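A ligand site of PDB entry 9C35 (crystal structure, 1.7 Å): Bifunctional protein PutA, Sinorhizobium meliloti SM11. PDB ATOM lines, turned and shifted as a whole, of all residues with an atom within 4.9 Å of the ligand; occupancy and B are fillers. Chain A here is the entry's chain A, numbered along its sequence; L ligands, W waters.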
ATOM      1  N   ASP A 308      -5.642  -1.994  -5.171  1.00  0.00           N
ATOM      2  CA  ASP A 308      -5.198  -2.458  -3.860  1.00  0.00           C
ATOM      3  C   ASP A 308      -5.983  -3.693  -3.468  1.00  0.00           C
ATOM      4  O   ASP A 308      -7.156  -3.861  -3.853  1.00  0.00           O
ATOM      5  CB  ASP A 308      -5.397  -1.373  -2.799  1.00  0.00           C
ATOM      6  CG  ASP A 308      -4.142  -0.524  -2.539  1.00  0.00           C
ATOM      7  OD1 ASP A 308      -3.112  -0.657  -3.263  1.00  0.00           O
ATOM      8  OD2 ASP A 308      -4.176   0.304  -1.586  1.00  0.00           O
ATOM      9  N   ALA A 309      -5.332  -4.569  -2.680  1.00  0.00           N
ATOM     10  CA  ALA A 309      -5.971  -5.776  -2.146  1.00  0.00           C
ATOM     11  C   ALA A 309      -6.567  -5.521  -0.762  1.00  0.00           C
ATOM     12  O   ALA A 309      -5.987  -4.816   0.068  1.00  0.00           O
ATOM     13  CB  ALA A 309      -4.990  -6.944  -2.064  1.00  0.00           C
ATOM     14  N   VAL A 340      -2.404  -5.812  -6.501  1.00  0.00           N
ATOM     15  CA  VAL A 340      -1.670  -6.245  -5.321  1.00  0.00           C
ATOM     16  C   VAL A 340      -1.971  -7.715  -5.054  1.00  0.00           C
ATOM     17  O   VAL A 340      -3.128  -8.169  -5.203  1.00  0.00           O
ATOM     18  CB  VAL A 340      -2.069  -5.398  -4.087  1.00  0.00           C
ATOM     19  CG1 VAL A 340      -1.414  -5.904  -2.801  1.00  0.00           C
ATOM     20  CG2 VAL A 340      -1.730  -3.919  -4.252  1.00  0.00           C
ATOM     21  N   GLN A 342      -1.243 -10.593  -1.776  1.00  0.00           N
ATOM     22  CA  GLN A 342      -0.945 -10.558  -0.341  1.00  0.00           C
ATOM     23  C   GLN A 342      -0.261 -11.861   0.036  1.00  0.00           C
ATOM     24  O   GLN A 342      -0.891 -12.922   0.026  1.00  0.00           O
ATOM     25  CB  GLN A 342      -2.202 -10.351   0.491  1.00  0.00           C
ATOM     26  CG  GLN A 342      -2.889  -9.037   0.280  1.00  0.00           C
ATOM     27  CD  GLN A 342      -4.375  -9.141   0.590  1.00  0.00           C
ATOM     28  OE1 GLN A 342      -5.071 -10.039   0.122  1.00  0.00           O
ATOM     29  NE2 GLN A 342      -4.862  -8.172   1.339  1.00  0.00           N
ATOM     30  N   TYR A 344       0.739 -12.993   2.852  1.00  0.00           N
ATOM     31  CA  TYR A 344       0.281 -13.728   4.016  1.00  0.00           C
ATOM     32  C   TYR A 344      -0.926 -14.609   3.711  1.00  0.00           C
ATOM     33  O   TYR A 344      -1.484 -15.206   4.626  1.00  0.00           O
ATOM     34  CB  TYR A 344      -0.006 -12.768   5.173  1.00  0.00           C
ATOM     35  CG  TYR A 344      -1.257 -11.884   5.144  1.00  0.00           C
ATOM     36  CD1 TYR A 344      -2.070 -11.793   4.046  1.00  0.00           C
ATOM     37  CD2 TYR A 344      -1.591 -11.101   6.252  1.00  0.00           C
ATOM     38  CE1 TYR A 344      -3.189 -10.977   4.022  1.00  0.00           C
ATOM     39  CE2 TYR A 344      -2.725 -10.262   6.262  1.00  0.00           C
ATOM     40  CZ  TYR A 344      -3.524 -10.222   5.147  1.00  0.00           C
ATOM     41  OH  TYR A 344      -4.627  -9.418   5.131  1.00  0.00           O
ATOM     42  N   ARG A 369       2.234  -5.890  -7.436  1.00  0.00           N
ATOM     43  CA  ARG A 369       2.773  -5.358  -6.190  1.00  0.00           C
ATOM     44  C   ARG A 369       2.579  -6.480  -5.173  1.00  0.00           C
ATOM     45  O   ARG A 369       1.448  -6.828  -4.846  1.00  0.00           O
ATOM     46  CB  ARG A 369       2.052  -4.094  -5.729  1.00  0.00           C
ATOM     47  CG  ARG A 369       2.659  -3.496  -4.485  1.00  0.00           C
ATOM     48  CD  ARG A 369       1.747  -2.521  -3.771  1.00  0.00           C
ATOM     49  NE  ARG A 369       1.582  -1.278  -4.521  1.00  0.00           N
ATOM     50  CZ  ARG A 369       0.712  -0.322  -4.226  1.00  0.00           C
ATOM     51  NH1 ARG A 369      -0.152  -0.466  -3.224  1.00  0.00           N
ATOM     52  NH2 ARG A 369       0.707   0.796  -4.960  1.00  0.00           N
ATOM     53  N   VAL A 371       2.803  -7.594  -1.534  1.00  0.00           N
ATOM     54  CA  VAL A 371       2.839  -7.097  -0.162  1.00  0.00           C
ATOM     55  C   VAL A 371       2.738  -8.294   0.768  1.00  0.00           C
ATOM     56  O   VAL A 371       2.584  -9.444   0.331  1.00  0.00           O
ATOM     57  CB  VAL A 371       1.726  -6.082   0.135  1.00  0.00           C
ATOM     58  CG1 VAL A 371       1.848  -4.880  -0.792  1.00  0.00           C
ATOM     59  CG2 VAL A 371       0.357  -6.710   0.035  1.00  0.00           C
ATOM     60  N   LYS A 372       2.867  -8.047   2.067  1.00  0.00           N
ATOM     61  CA  LYS A 372       2.610  -9.163   2.973  1.00  0.00           C
ATOM     62  C   LYS A 372       1.126  -9.220   3.313  1.00  0.00           C
ATOM     63  O   LYS A 372       0.453 -10.196   2.966  1.00  0.00           O
ATOM     64  CB  LYS A 372       3.520  -9.087   4.199  1.00  0.00           C
ATOM     65  CG  LYS A 372       4.903  -9.630   3.779  1.00  0.00           C
ATOM     66  CD  LYS A 372       5.990  -9.569   4.859  1.00  0.00           C
ATOM     67  CE  LYS A 372       7.358  -9.770   4.167  1.00  0.00           C
ATOM     68  NZ  LYS A 372       8.516  -9.928   5.088  1.00  0.00           N
ATOM     69  N   GLY A 373       0.590  -8.177   3.884  1.00  0.00           N
ATOM     70  CA  GLY A 373      -0.856  -8.011   4.006  1.00  0.00           C
ATOM     71  C   GLY A 373      -1.175  -7.273   5.287  1.00  0.00           C
ATOM     72  O   GLY A 373      -0.486  -7.367   6.295  1.00  0.00           O
ATOM     73  N   ALA A 374      -2.297  -6.532   5.251  1.00  0.00           N
ATOM     74  CA  ALA A 374      -2.606  -5.549   6.281  1.00  0.00           C
ATOM     75  C   ALA A 374      -3.828  -5.852   7.146  1.00  0.00           C
ATOM     76  O   ALA A 374      -4.138  -5.043   8.041  1.00  0.00           O
ATOM     77  CB  ALA A 374      -2.823  -4.164   5.641  1.00  0.00           C
ATOM     78  N   TYR A 375      -4.536  -6.964   6.921  1.00  0.00           N
ATOM     79  CA  TYR A 375      -5.778  -7.258   7.642  1.00  0.00           C
ATOM     80  C   TYR A 375      -5.665  -8.514   8.521  1.00  0.00           C
ATOM     81  O   TYR A 375      -6.661  -9.186   8.793  1.00  0.00           O
ATOM     82  CB  TYR A 375      -6.938  -7.416   6.666  1.00  0.00           C
ATOM     83  CG  TYR A 375      -7.124  -6.249   5.709  1.00  0.00           C
ATOM     84  CD1 TYR A 375      -6.407  -6.207   4.508  1.00  0.00           C
ATOM     85  CD2 TYR A 375      -8.032  -5.269   5.967  1.00  0.00           C
ATOM     86  CE1 TYR A 375      -6.603  -5.141   3.618  1.00  0.00           C
ATOM     87  CE2 TYR A 375      -8.215  -4.199   5.110  1.00  0.00           C
ATOM     88  CZ  TYR A 375      -7.509  -4.153   3.916  1.00  0.00           C
ATOM     89  OH  TYR A 375      -7.716  -3.086   3.065  1.00  0.00           O
ATOM     90  N   TRP A 376      -4.466  -8.786   9.025  1.00  0.00           N
ATOM     91  CA  TRP A 376      -4.218 -10.093   9.620  1.00  0.00           C
ATOM     92  C   TRP A 376      -5.154 -10.385  10.792  1.00  0.00           C
ATOM     93  O   TRP A 376      -5.821 -11.430  10.813  1.00  0.00           O
ATOM     94  CB  TRP A 376      -2.768 -10.199  10.086  1.00  0.00           C
ATOM     95  CG  TRP A 376      -2.503 -11.546  10.663  1.00  0.00           C
ATOM     96  CD1 TRP A 376      -2.312 -12.715   9.972  1.00  0.00           C
ATOM     97  CD2 TRP A 376      -2.407 -11.883  12.063  1.00  0.00           C
ATOM     98  NE1 TRP A 376      -2.112 -13.763  10.859  1.00  0.00           N
ATOM     99  CE2 TRP A 376      -2.166 -13.268  12.137  1.00  0.00           C
ATOM    100  CE3 TRP A 376      -2.506 -11.141  13.246  1.00  0.00           C
ATOM    101  CZ2 TRP A 376      -2.009 -13.930  13.369  1.00  0.00           C
ATOM    102  CZ3 TRP A 376      -2.352 -11.796  14.455  1.00  0.00           C
ATOM    103  CH2 TRP A 376      -2.104 -13.177  14.508  1.00  0.00           C
ATOM    104  N   PHE A 394      -1.696 -17.174   6.819  1.00  0.00           N
ATOM    105  CA  PHE A 394      -0.815 -17.923   7.722  1.00  0.00           C
ATOM    106  C   PHE A 394      -0.989 -17.387   9.152  1.00  0.00           C
ATOM    107  O   PHE A 394      -1.518 -16.299   9.364  1.00  0.00           O
ATOM    108  CB  PHE A 394       0.624 -17.829   7.235  1.00  0.00           C
ATOM    109  CG  PHE A 394       0.816 -18.386   5.836  1.00  0.00           C
ATOM    110  CD1 PHE A 394       0.633 -19.728   5.568  1.00  0.00           C
ATOM    111  CD2 PHE A 394       1.118 -17.545   4.779  1.00  0.00           C
ATOM    112  CE1 PHE A 394       0.779 -20.237   4.294  1.00  0.00           C
ATOM    113  CE2 PHE A 394       1.256 -18.016   3.525  1.00  0.00           C
ATOM    114  CZ  PHE A 394       1.089 -19.371   3.264  1.00  0.00           C
ATOM    115  N   THR A 395      -0.593 -18.195  10.139  1.00  0.00           N
ATOM    116  CA  THR A 395      -0.672 -17.796  11.541  1.00  0.00           C
ATOM    117  C   THR A 395       0.689 -17.588  12.192  1.00  0.00           C
ATOM    118  O   THR A 395       0.753 -17.180  13.360  1.00  0.00           O
ATOM    119  CB  THR A 395      -1.434 -18.837  12.375  1.00  0.00           C
ATOM    120  OG1 THR A 395      -0.712 -20.075  12.373  1.00  0.00           O
ATOM    121  CG2 THR A 395      -2.859 -19.036  11.845  1.00  0.00           C
ATOM    122  N   ARG A 396       1.776 -17.859  11.496  1.00  0.00           N
ATOM    123  CA  ARG A 396       3.104 -17.507  11.964  1.00  0.00           C
ATOM    124  C   ARG A 396       3.699 -16.489  10.992  1.00  0.00           C
ATOM    125  O   ARG A 396       3.699 -16.712   9.780  1.00  0.00           O
ATOM    126  CB  ARG A 396       3.995 -18.734  12.051  1.00  0.00           C
ATOM    127  CG  ARG A 396       3.413 -19.887  12.839  1.00  0.00           C
ATOM    128  CD  ARG A 396       4.509 -20.835  13.356  1.00  0.00           C
ATOM    129  NE  ARG A 396       3.994 -21.805  14.313  1.00  0.00           N
ATOM    130  CZ  ARG A 396       4.754 -22.536  15.131  1.00  0.00           C
ATOM    131  NH1 ARG A 396       6.068 -22.394  15.153  1.00  0.00           N
ATOM    132  NH2 ARG A 396       4.185 -23.439  15.920  1.00  0.00           N
ATOM    133  N   LYS A 397       4.220 -15.397  11.550  1.00  0.00           N
ATOM    134  CA  LYS A 397       4.829 -14.352  10.733  1.00  0.00           C
ATOM    135  C   LYS A 397       5.964 -14.900   9.876  1.00  0.00           C
ATOM    136  O   LYS A 397       6.175 -14.429   8.735  1.00  0.00           O
ATOM    137  CB  LYS A 397       5.309 -13.233  11.645  1.00  0.00           C
ATOM    138  CG  LYS A 397       5.626 -11.943  10.962  1.00  0.00           C
ATOM    139  CD  LYS A 397       7.095 -11.883  10.565  1.00  0.00           C
ATOM    140  CE  LYS A 397       7.360 -10.615   9.749  1.00  0.00           C
ATOM    141  NZ  LYS A 397       8.764 -10.574   9.268  1.00  0.00           N
ATOM    142  N   THR A 400       4.676 -16.082   6.584  1.00  0.00           N
ATOM    143  CA  THR A 400       4.487 -15.003   5.607  1.00  0.00           C
ATOM    144  C   THR A 400       5.800 -14.639   4.916  1.00  0.00           C
ATOM    145  O   THR A 400       5.851 -14.426   3.687  1.00  0.00           O
ATOM    146  CB  THR A 400       3.844 -13.813   6.295  1.00  0.00           C
ATOM    147  OG1 THR A 400       2.539 -14.195   6.792  1.00  0.00           O
ATOM    148  CG2 THR A 400       3.714 -12.592   5.369  1.00  0.00           C
ATOM    149  N   ASP A 401       6.906 -14.636   5.666  1.00  0.00           N
ATOM    150  CA  ASP A 401       8.181 -14.262   5.080  1.00  0.00           C
ATOM    151  C   ASP A 401       8.618 -15.275   4.024  1.00  0.00           C
ATOM    152  O   ASP A 401       9.096 -14.885   2.965  1.00  0.00           O
ATOM    153  CB  ASP A 401       9.274 -14.141   6.146  1.00  0.00           C
ATOM    154  CG  ASP A 401       9.068 -12.949   7.093  1.00  0.00           C
ATOM    155  OD1 ASP A 401       8.426 -11.938   6.749  1.00  0.00           O
ATOM    156  OD2 ASP A 401       9.589 -13.027   8.217  1.00  0.00           O
ATOM    157  N   ALA A 423       7.137  -4.687  -2.334  1.00  0.00           N
ATOM    158  CA  ALA A 423       6.832  -3.742  -1.273  1.00  0.00           C
ATOM    159  C   ALA A 423       7.290  -4.361   0.018  1.00  0.00           C
ATOM    160  O   ALA A 423       6.680  -5.334   0.489  1.00  0.00           O
ATOM    161  CB  ALA A 423       5.336  -3.418  -1.224  1.00  0.00           C
ATOM    162  N   THR A 424       8.380  -3.848   0.591  1.00  0.00           N
ATOM    163  CA  THR A 424       8.798  -4.312   1.918  1.00  0.00           C
ATOM    164  C   THR A 424       9.713  -3.279   2.581  1.00  0.00           C
ATOM    165  O   THR A 424      10.410  -2.530   1.893  1.00  0.00           O
ATOM    166  CB  THR A 424       9.504  -5.677   1.839  1.00  0.00           C
ATOM    167  OG1 THR A 424       9.818  -6.157   3.146  1.00  0.00           O
ATOM    168  CG2 THR A 424      10.809  -5.586   1.037  1.00  0.00           C
ATOM    169  N   HIS A 425       9.638  -3.220   3.924  1.00  0.00           N
ATOM    170  CA  HIS A 425      10.613  -2.492   4.733  1.00  0.00           C
ATOM    171  C   HIS A 425      11.612  -3.423   5.414  1.00  0.00           C
ATOM    172  O   HIS A 425      12.483  -2.954   6.160  1.00  0.00           O
ATOM    173  CB  HIS A 425       9.914  -1.666   5.809  1.00  0.00           C
ATOM    174  CG  HIS A 425       9.063  -0.572   5.257  1.00  0.00           C
ATOM    175  ND1 HIS A 425       7.799  -0.296   5.721  1.00  0.00           N
ATOM    176  CD2 HIS A 425       9.294   0.299   4.250  1.00  0.00           C
ATOM    177  CE1 HIS A 425       7.288   0.707   5.028  1.00  0.00           C
ATOM    178  NE2 HIS A 425       8.166   1.089   4.126  1.00  0.00           N
ATOM    179  N   ASN A 426      11.491  -4.725   5.224  1.00  0.00           N
ATOM    180  CA  ASN A 426      12.321  -5.705   5.900  1.00  0.00           C
ATOM    181  C   ASN A 426      13.641  -5.837   5.169  1.00  0.00           C
ATOM    182  O   ASN A 426      13.678  -6.320   4.033  1.00  0.00           O
ATOM    183  CB  ASN A 426      11.581  -7.029   5.955  1.00  0.00           C
ATOM    184  CG  ASN A 426      12.313  -8.056   6.790  1.00  0.00           C
ATOM    185  OD1 ASN A 426      13.538  -8.193   6.715  1.00  0.00           O
ATOM    186  ND2 ASN A 426      11.550  -8.781   7.616  1.00  0.00           N
ATOM    187  N   GLN A 449       9.400  -1.059  -3.395  1.00  0.00           N
ATOM    188  CA  GLN A 449       8.416  -0.084  -2.951  1.00  0.00           C
ATOM    189  C   GLN A 449       8.458   0.020  -1.424  1.00  0.00           C
ATOM    190  O   GLN A 449       8.732  -0.960  -0.738  1.00  0.00           O
ATOM    191  CB  GLN A 449       6.988  -0.470  -3.360  1.00  0.00           C
ATOM    192  CG  GLN A 449       6.788  -0.616  -4.849  1.00  0.00           C
ATOM    193  CD  GLN A 449       5.345  -0.543  -5.253  1.00  0.00           C
ATOM    194  OE1 GLN A 449       4.439  -0.667  -4.424  1.00  0.00           O
ATOM    195  NE2 GLN A 449       5.093  -0.317  -6.532  1.00  0.00           N
ATOM    196  N   CYS A 450       8.138   1.219  -0.928  1.00  0.00           N
ATOM    197  CA  CYS A 450       8.094   1.530   0.505  1.00  0.00           C
ATOM    198  C   CYS A 450       7.014   2.561   0.774  1.00  0.00           C
ATOM    199  O   CYS A 450       6.416   3.121  -0.153  1.00  0.00           O
ATOM    200  CB  CYS A 450       9.431   2.066   1.013  1.00  0.00           C
ATOM    201  SG  CYS A 450       9.790   3.785   0.483  1.00  0.00           S
ATOM    202  N   LEU A 451       6.756   2.830   2.063  1.00  0.00           N
ATOM    203  CA  LEU A 451       5.719   3.744   2.499  1.00  0.00           C
ATOM    204  C   LEU A 451       6.337   5.080   2.879  1.00  0.00           C
ATOM    205  O   LEU A 451       7.385   5.121   3.522  1.00  0.00           O
ATOM    206  CB  LEU A 451       4.931   3.205   3.705  1.00  0.00           C
ATOM    207  N   TYR A 475       4.989   4.886  -1.729  1.00  0.00           N
ATOM    208  CA  TYR A 475       3.536   4.903  -1.623  1.00  0.00           C
ATOM    209  C   TYR A 475       3.108   6.021  -0.666  1.00  0.00           C
ATOM    210  O   TYR A 475       3.446   6.019   0.523  1.00  0.00           O
ATOM    211  CB  TYR A 475       3.102   3.506  -1.172  1.00  0.00           C
ATOM    212  CG  TYR A 475       1.621   3.217  -1.100  1.00  0.00           C
ATOM    213  CD1 TYR A 475       0.933   2.751  -2.217  1.00  0.00           C
ATOM    214  CD2 TYR A 475       0.921   3.310   0.112  1.00  0.00           C
ATOM    215  CE1 TYR A 475      -0.431   2.449  -2.156  1.00  0.00           C
ATOM    216  CE2 TYR A 475      -0.438   3.010   0.194  1.00  0.00           C
ATOM    217  CZ  TYR A 475      -1.104   2.565  -0.945  1.00  0.00           C
ATOM    218  OH  TYR A 475      -2.447   2.256  -0.888  1.00  0.00           O
ATOM    219  N   SER A 499       6.258  -8.351  16.424  1.00  0.00           N
ATOM    220  CA  SER A 499       6.943  -9.179  15.430  1.00  0.00           C
ATOM    221  C   SER A 499       7.327  -8.421  14.170  1.00  0.00           C
ATOM    222  O   SER A 499       7.972  -9.006  13.284  1.00  0.00           O
ATOM    223  CB  SER A 499       6.056 -10.375  15.058  1.00  0.00           C
ATOM    224  OG  SER A 499       4.744  -9.937  14.707  1.00  0.00           O
ATOM    225  N   SER A 500       6.978  -7.141  14.056  1.00  0.00           N
ATOM    226  CA  SER A 500       7.303  -6.350  12.879  1.00  0.00           C
ATOM    227  C   SER A 500       8.794  -6.028  12.832  1.00  0.00           C
ATOM    228  O   SER A 500       9.397  -5.624  13.830  1.00  0.00           O
ATOM    229  CB  SER A 500       6.481  -5.059  12.898  1.00  0.00           C
ATOM    230  N   PHE A 501       9.408  -6.197  11.642  1.00  0.00           N
ATOM    231  CA  PHE A 501      10.790  -5.772  11.427  1.00  0.00           C
ATOM    232  C   PHE A 501      11.006  -4.330  11.877  1.00  0.00           C
ATOM    233  O   PHE A 501      12.012  -4.014  12.514  1.00  0.00           O
ATOM    234  CB  PHE A 501      11.191  -5.926   9.950  1.00  0.00           C
ATOM    235  CG  PHE A 501      12.612  -5.498   9.638  1.00  0.00           C
ATOM    236  CD1 PHE A 501      12.909  -4.156   9.360  1.00  0.00           C
ATOM    237  CD2 PHE A 501      13.640  -6.421   9.636  1.00  0.00           C
ATOM    238  CE1 PHE A 501      14.226  -3.765   9.086  1.00  0.00           C
ATOM    239  CE2 PHE A 501      14.942  -6.035   9.370  1.00  0.00           C
ATOM    240  CZ  PHE A 501      15.235  -4.700   9.104  1.00  0.00           C
ATOM    241  N   VAL A 502      10.092  -3.426  11.508  1.00  0.00           N
ATOM    242  CA  VAL A 502      10.224  -2.031  11.920  1.00  0.00           C
ATOM    243  C   VAL A 502      10.349  -1.954  13.431  1.00  0.00           C
ATOM    244  O   VAL A 502      11.164  -1.191  13.972  1.00  0.00           O
ATOM    245  CB  VAL A 502       9.050  -1.201  11.394  1.00  0.00           C
ATOM    246  N   HIS A 533       0.336 -21.672  14.549  1.00  0.00           N
ATOM    247  CA  HIS A 533       0.729 -20.994  15.787  1.00  0.00           C
ATOM    248  C   HIS A 533       0.089 -21.668  16.999  1.00  0.00           C
ATOM    249  O   HIS A 533      -1.099 -22.004  16.981  1.00  0.00           O
ATOM    250  CB  HIS A 533       0.287 -19.528  15.731  1.00  0.00           C
ATOM    251  CG  HIS A 533       0.932 -18.638  16.739  1.00  0.00           C
ATOM    252  ND1 HIS A 533       0.622 -18.683  18.076  1.00  0.00           N
ATOM    253  CD2 HIS A 533       1.830 -17.630  16.591  1.00  0.00           C
ATOM    254  CE1 HIS A 533       1.321 -17.771  18.732  1.00  0.00           C
ATOM    255  NE2 HIS A 533       2.053 -17.111  17.852  1.00  0.00           N
HETATM  256  P1  LIG L   1       7.512  -7.196   8.311  1.00  0.00           P
HETATM  257  O1  LIG L   1       7.673  -6.964   9.854  1.00  0.00           O
HETATM  258  O2  LIG L   1       8.528  -7.892   7.602  1.00  0.00           O
HETATM  259  O3  LIG L   1       6.338  -8.037   7.993  1.00  0.00           O
HETATM  260  C1  LIG L   1       5.183  -7.860   8.814  1.00  0.00           C
HETATM  261  C2  LIG L   1       3.986  -8.547   8.219  1.00  0.00           C
HETATM  262  O4  LIG L   1       3.923  -9.900   8.564  1.00  0.00           O
HETATM  263  C3  LIG L   1       2.640  -8.032   8.602  1.00  0.00           C
HETATM  264  O5  LIG L   1       2.249  -6.939   7.892  1.00  0.00           O
HETATM  265  C4  LIG L   1       1.708  -9.136   8.313  1.00  0.00           C
HETATM  266  O6  LIG L   1       1.313  -9.146   6.976  1.00  0.00           O
HETATM  267  C5  LIG L   1       2.551 -10.309   8.608  1.00  0.00           C
HETATM  268  N1  LIG L   1       2.357 -10.959   9.884  1.00  0.00           N
HETATM  269  C6  LIG L   1       2.567 -10.463  11.169  1.00  0.00           C
HETATM  270  N2  LIG L   1       2.294 -11.429  12.064  1.00  0.00           N
HETATM  271  C7  LIG L   1       1.862 -12.574  11.413  1.00  0.00           C
HETATM  272  C8  LIG L   1       1.469 -13.839  11.786  1.00  0.00           C
HETATM  273  N3  LIG L   1       1.389 -14.226  13.169  1.00  0.00           N
HETATM  274  N4  LIG L   1       1.131 -14.738  10.851  1.00  0.00           N
HETATM  275  C9  LIG L   1       1.173 -14.470   9.511  1.00  0.00           C
HETATM  276  N5  LIG L   1       1.580 -13.238   9.097  1.00  0.00           N
HETATM  277  C10 LIG L   1       1.916 -12.304   9.991  1.00  0.00           C
HETATM  278  N6  LIG L   1      -1.160  -4.505   2.409  1.00  0.00           N
HETATM  279  C11 LIG L   1      -2.403  -4.943   1.834  1.00  0.00           C
HETATM  280  O7  LIG L   1      -3.051  -6.003   2.403  1.00  0.00           O
HETATM  281  N7  LIG L   1      -2.965  -4.308   0.695  1.00  0.00           N
HETATM  282  C12 LIG L   1      -2.286  -3.212   0.082  1.00  0.00           C
HETATM  283  O8  LIG L   1      -2.890  -2.646  -1.039  1.00  0.00           O
HETATM  284  C13 LIG L   1      -0.967  -2.755   0.701  1.00  0.00           C
HETATM  285  N8  LIG L   1      -0.183  -1.696   0.101  1.00  0.00           N
HETATM  286  C14 LIG L   1       1.220  -1.556   0.514  1.00  0.00           C
HETATM  287  C15 LIG L   1       2.125  -0.687  -0.285  1.00  0.00           C
HETATM  288  C16 LIG L   1       3.475  -0.524   0.110  1.00  0.00           C
HETATM  289  C17 LIG L   1       4.406   0.358  -0.696  1.00  0.00           C
HETATM  290  C18 LIG L   1       4.012  -1.202   1.265  1.00  0.00           C
HETATM  291  C19 LIG L   1       5.473  -1.003   1.634  1.00  0.00           C
HETATM  292  C20 LIG L   1       3.155  -2.038   2.035  1.00  0.00           C
HETATM  293  C21 LIG L   1       1.725  -2.203   1.622  1.00  0.00           C
HETATM  294  N9  LIG L   1       0.849  -3.051   2.411  1.00  0.00           N
HETATM  295  C22 LIG L   1      -0.444  -3.367   1.846  1.00  0.00           C
HETATM  296  C23 LIG L   1       1.233  -3.489   3.765  1.00  0.00           C
HETATM  297  C24 LIG L   1       2.083  -4.711   3.926  1.00  0.00           C
HETATM  298  O9  LIG L   1       1.267  -5.778   3.559  1.00  0.00           O
HETATM  299  C25 LIG L   1       2.556  -5.002   5.348  1.00  0.00           C
HETATM  300  O10 LIG L   1       1.434  -5.028   6.155  1.00  0.00           O
HETATM  301  C26 LIG L   1       3.542  -3.999   5.961  1.00  0.00           C
HETATM  302  O11 LIG L   1       4.028  -3.190   4.944  1.00  0.00           O
HETATM  303  C27 LIG L   1       4.672  -4.652   6.738  1.00  0.00           C
HETATM  304  O12 LIG L   1       5.380  -5.571   5.964  1.00  0.00           O
HETATM  305  P2  LIG L   1       6.995  -5.670   5.937  1.00  0.00           P
HETATM  306  O13 LIG L   1       7.633  -6.568   4.792  1.00  0.00           O
HETATM  307  O14 LIG L   1       7.287  -4.132   5.904  1.00  0.00           O
HETATM  308  O15 LIG L   1       7.423  -5.933   7.499  1.00  0.00           O
HETATM  309  O   HOH W   1       5.218  -6.212   2.844  1.00  0.00           O
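O9 of the ligand sits at hydrogen-bond distance from N of Gly 373, at 2.5 Å. The backbone carbonyl oxygen (O) of Gly 373 is in hydrogen-bond range of an oxygen (O6) of the ligand (2.6 Å). The backbone NH (N) of Phe 501 lies within hydrogen-bond range of an oxygen (O1) of the ligand, at 2.6 Å. N5 of the ligand lies within hydrogen-bond range of OG1 of Thr 400 (2.7 Å). OG1 of Thr 424 sits at hydrogen-bond distance from O13 of the ligand (2.8 Å). The backbone NH of Ala 374 is in hydrogen-bond range of an oxygen (O7) of the ligand. NE2 of Gln 342 lies within hydrogen-bond range of O7 of the ligand, at 3.0 Å. A nitrogen (N3) of the ligand lies within hydrogen-bond range of the backbone carbonyl oxygen (O) of Thr 395, at 3.0 Å. N4 of the ligand lies close to N of Arg 396, at 3.3 Å. A nitrogen (N7) of the ligand lies within hydrogen-bond range of the backbone carbonyl oxygen (O) of Ala 309. The side-chain amide nitrogen of Asn 426 lies within hydrogen-bond range of an oxygen (O2) of the ligand (3.2 Å). The backbone NH (N) of Lys 372 is in hydrogen-bond range of an oxygen (O9) of the ligand, at 3.2 Å. The side-chain amino group (NZ) of Lys 372 lies within salt-bridge range of an oxygen (O2) of the ligand. N of Lys 397 lies close to N4 of the ligand, 3.2 Å away. An oxygen (O2) of the ligand lies within salt-bridge range of the side-chain amino group of Lys 397, 3.2 Å away. N of His 425 sits at hydrogen-bond distance from O14 of the ligand (3.2 Å). N4 of the ligand lies within hydrogen-bond range of NE1 of Trp 376, at 3.4 Å.
The backbone carbonyl oxygen of Gln 449 sits at hydrogen-bond distance from the backbone NH of Thr 424, at 3.2 Å. OD2 of Asp 308 sits at hydrogen-bond distance from OH of Tyr 475 (2.7 Å). NZ of Lys 397 lies within salt-bridge range of OD2 of Asp 401 (2.8 Å). The backbone carbonyl oxygen (O) of Phe 394 is in hydrogen-bond range of the indole nitrogen (NE1) of Trp 376 (3.0 Å). N of Phe 394 is in hydrogen-bond range of O of Tyr 344 (3.0 Å). The backbone NH of Tyr 475 sits at hydrogen-bond distance from the backbone carbonyl oxygen of Cys 450, at 2.8 Å. NE of Arg 369 is in hydrogen-bond range of OE1 of Gln 449 (2.9 Å). The side-chain hydroxyl (OH) of Tyr 344 lies within hydrogen-bond range of the backbone NH (N) of Tyr 375 (3.0 Å).
The side-chain carboxylate (OD1) of Asp 308 lies close to an oxygen (O8) of the ligand, 3.0 Å away. The backbone carbonyl oxygen (O) of Phe 394 sits close to a nitrogen (N4) of the ligand, at 3.4 Å. Val 340 touches the ligand. Tyr 344 touches the ligand (CD2 to O6, 3.6 Å). NH1 of Arg 369 touches N8 of the ligand (3.5 Å). CB of Val 371 touches O9 of the ligand (3.5 Å). CE1 of Tyr 375 touches O7 of the ligand, 3.9 Å away. Ala 423 touches the ligand (CB to C18, 3.6 Å). Gln 449 touches the ligand. Cys 450 touches the ligand. Tyr 475 touches the ligand. Ser 499 touches the ligand (OG to N2, 3.9 Å). Ser 500 touches the ligand. Hydrophobic or aromatic side chains that line the ligand: Val 340, Tyr 344, Val 371, Ala 374, Tyr 375, Trp 376, Ala 423, His 425, Tyr 475 and Phe 501.
Water W1 lies within hydrogen-bond range of O of Ala 423 (2.9 Å), N of Lys 372 (3.1 Å) and O13 of the ligand (3.1 Å).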
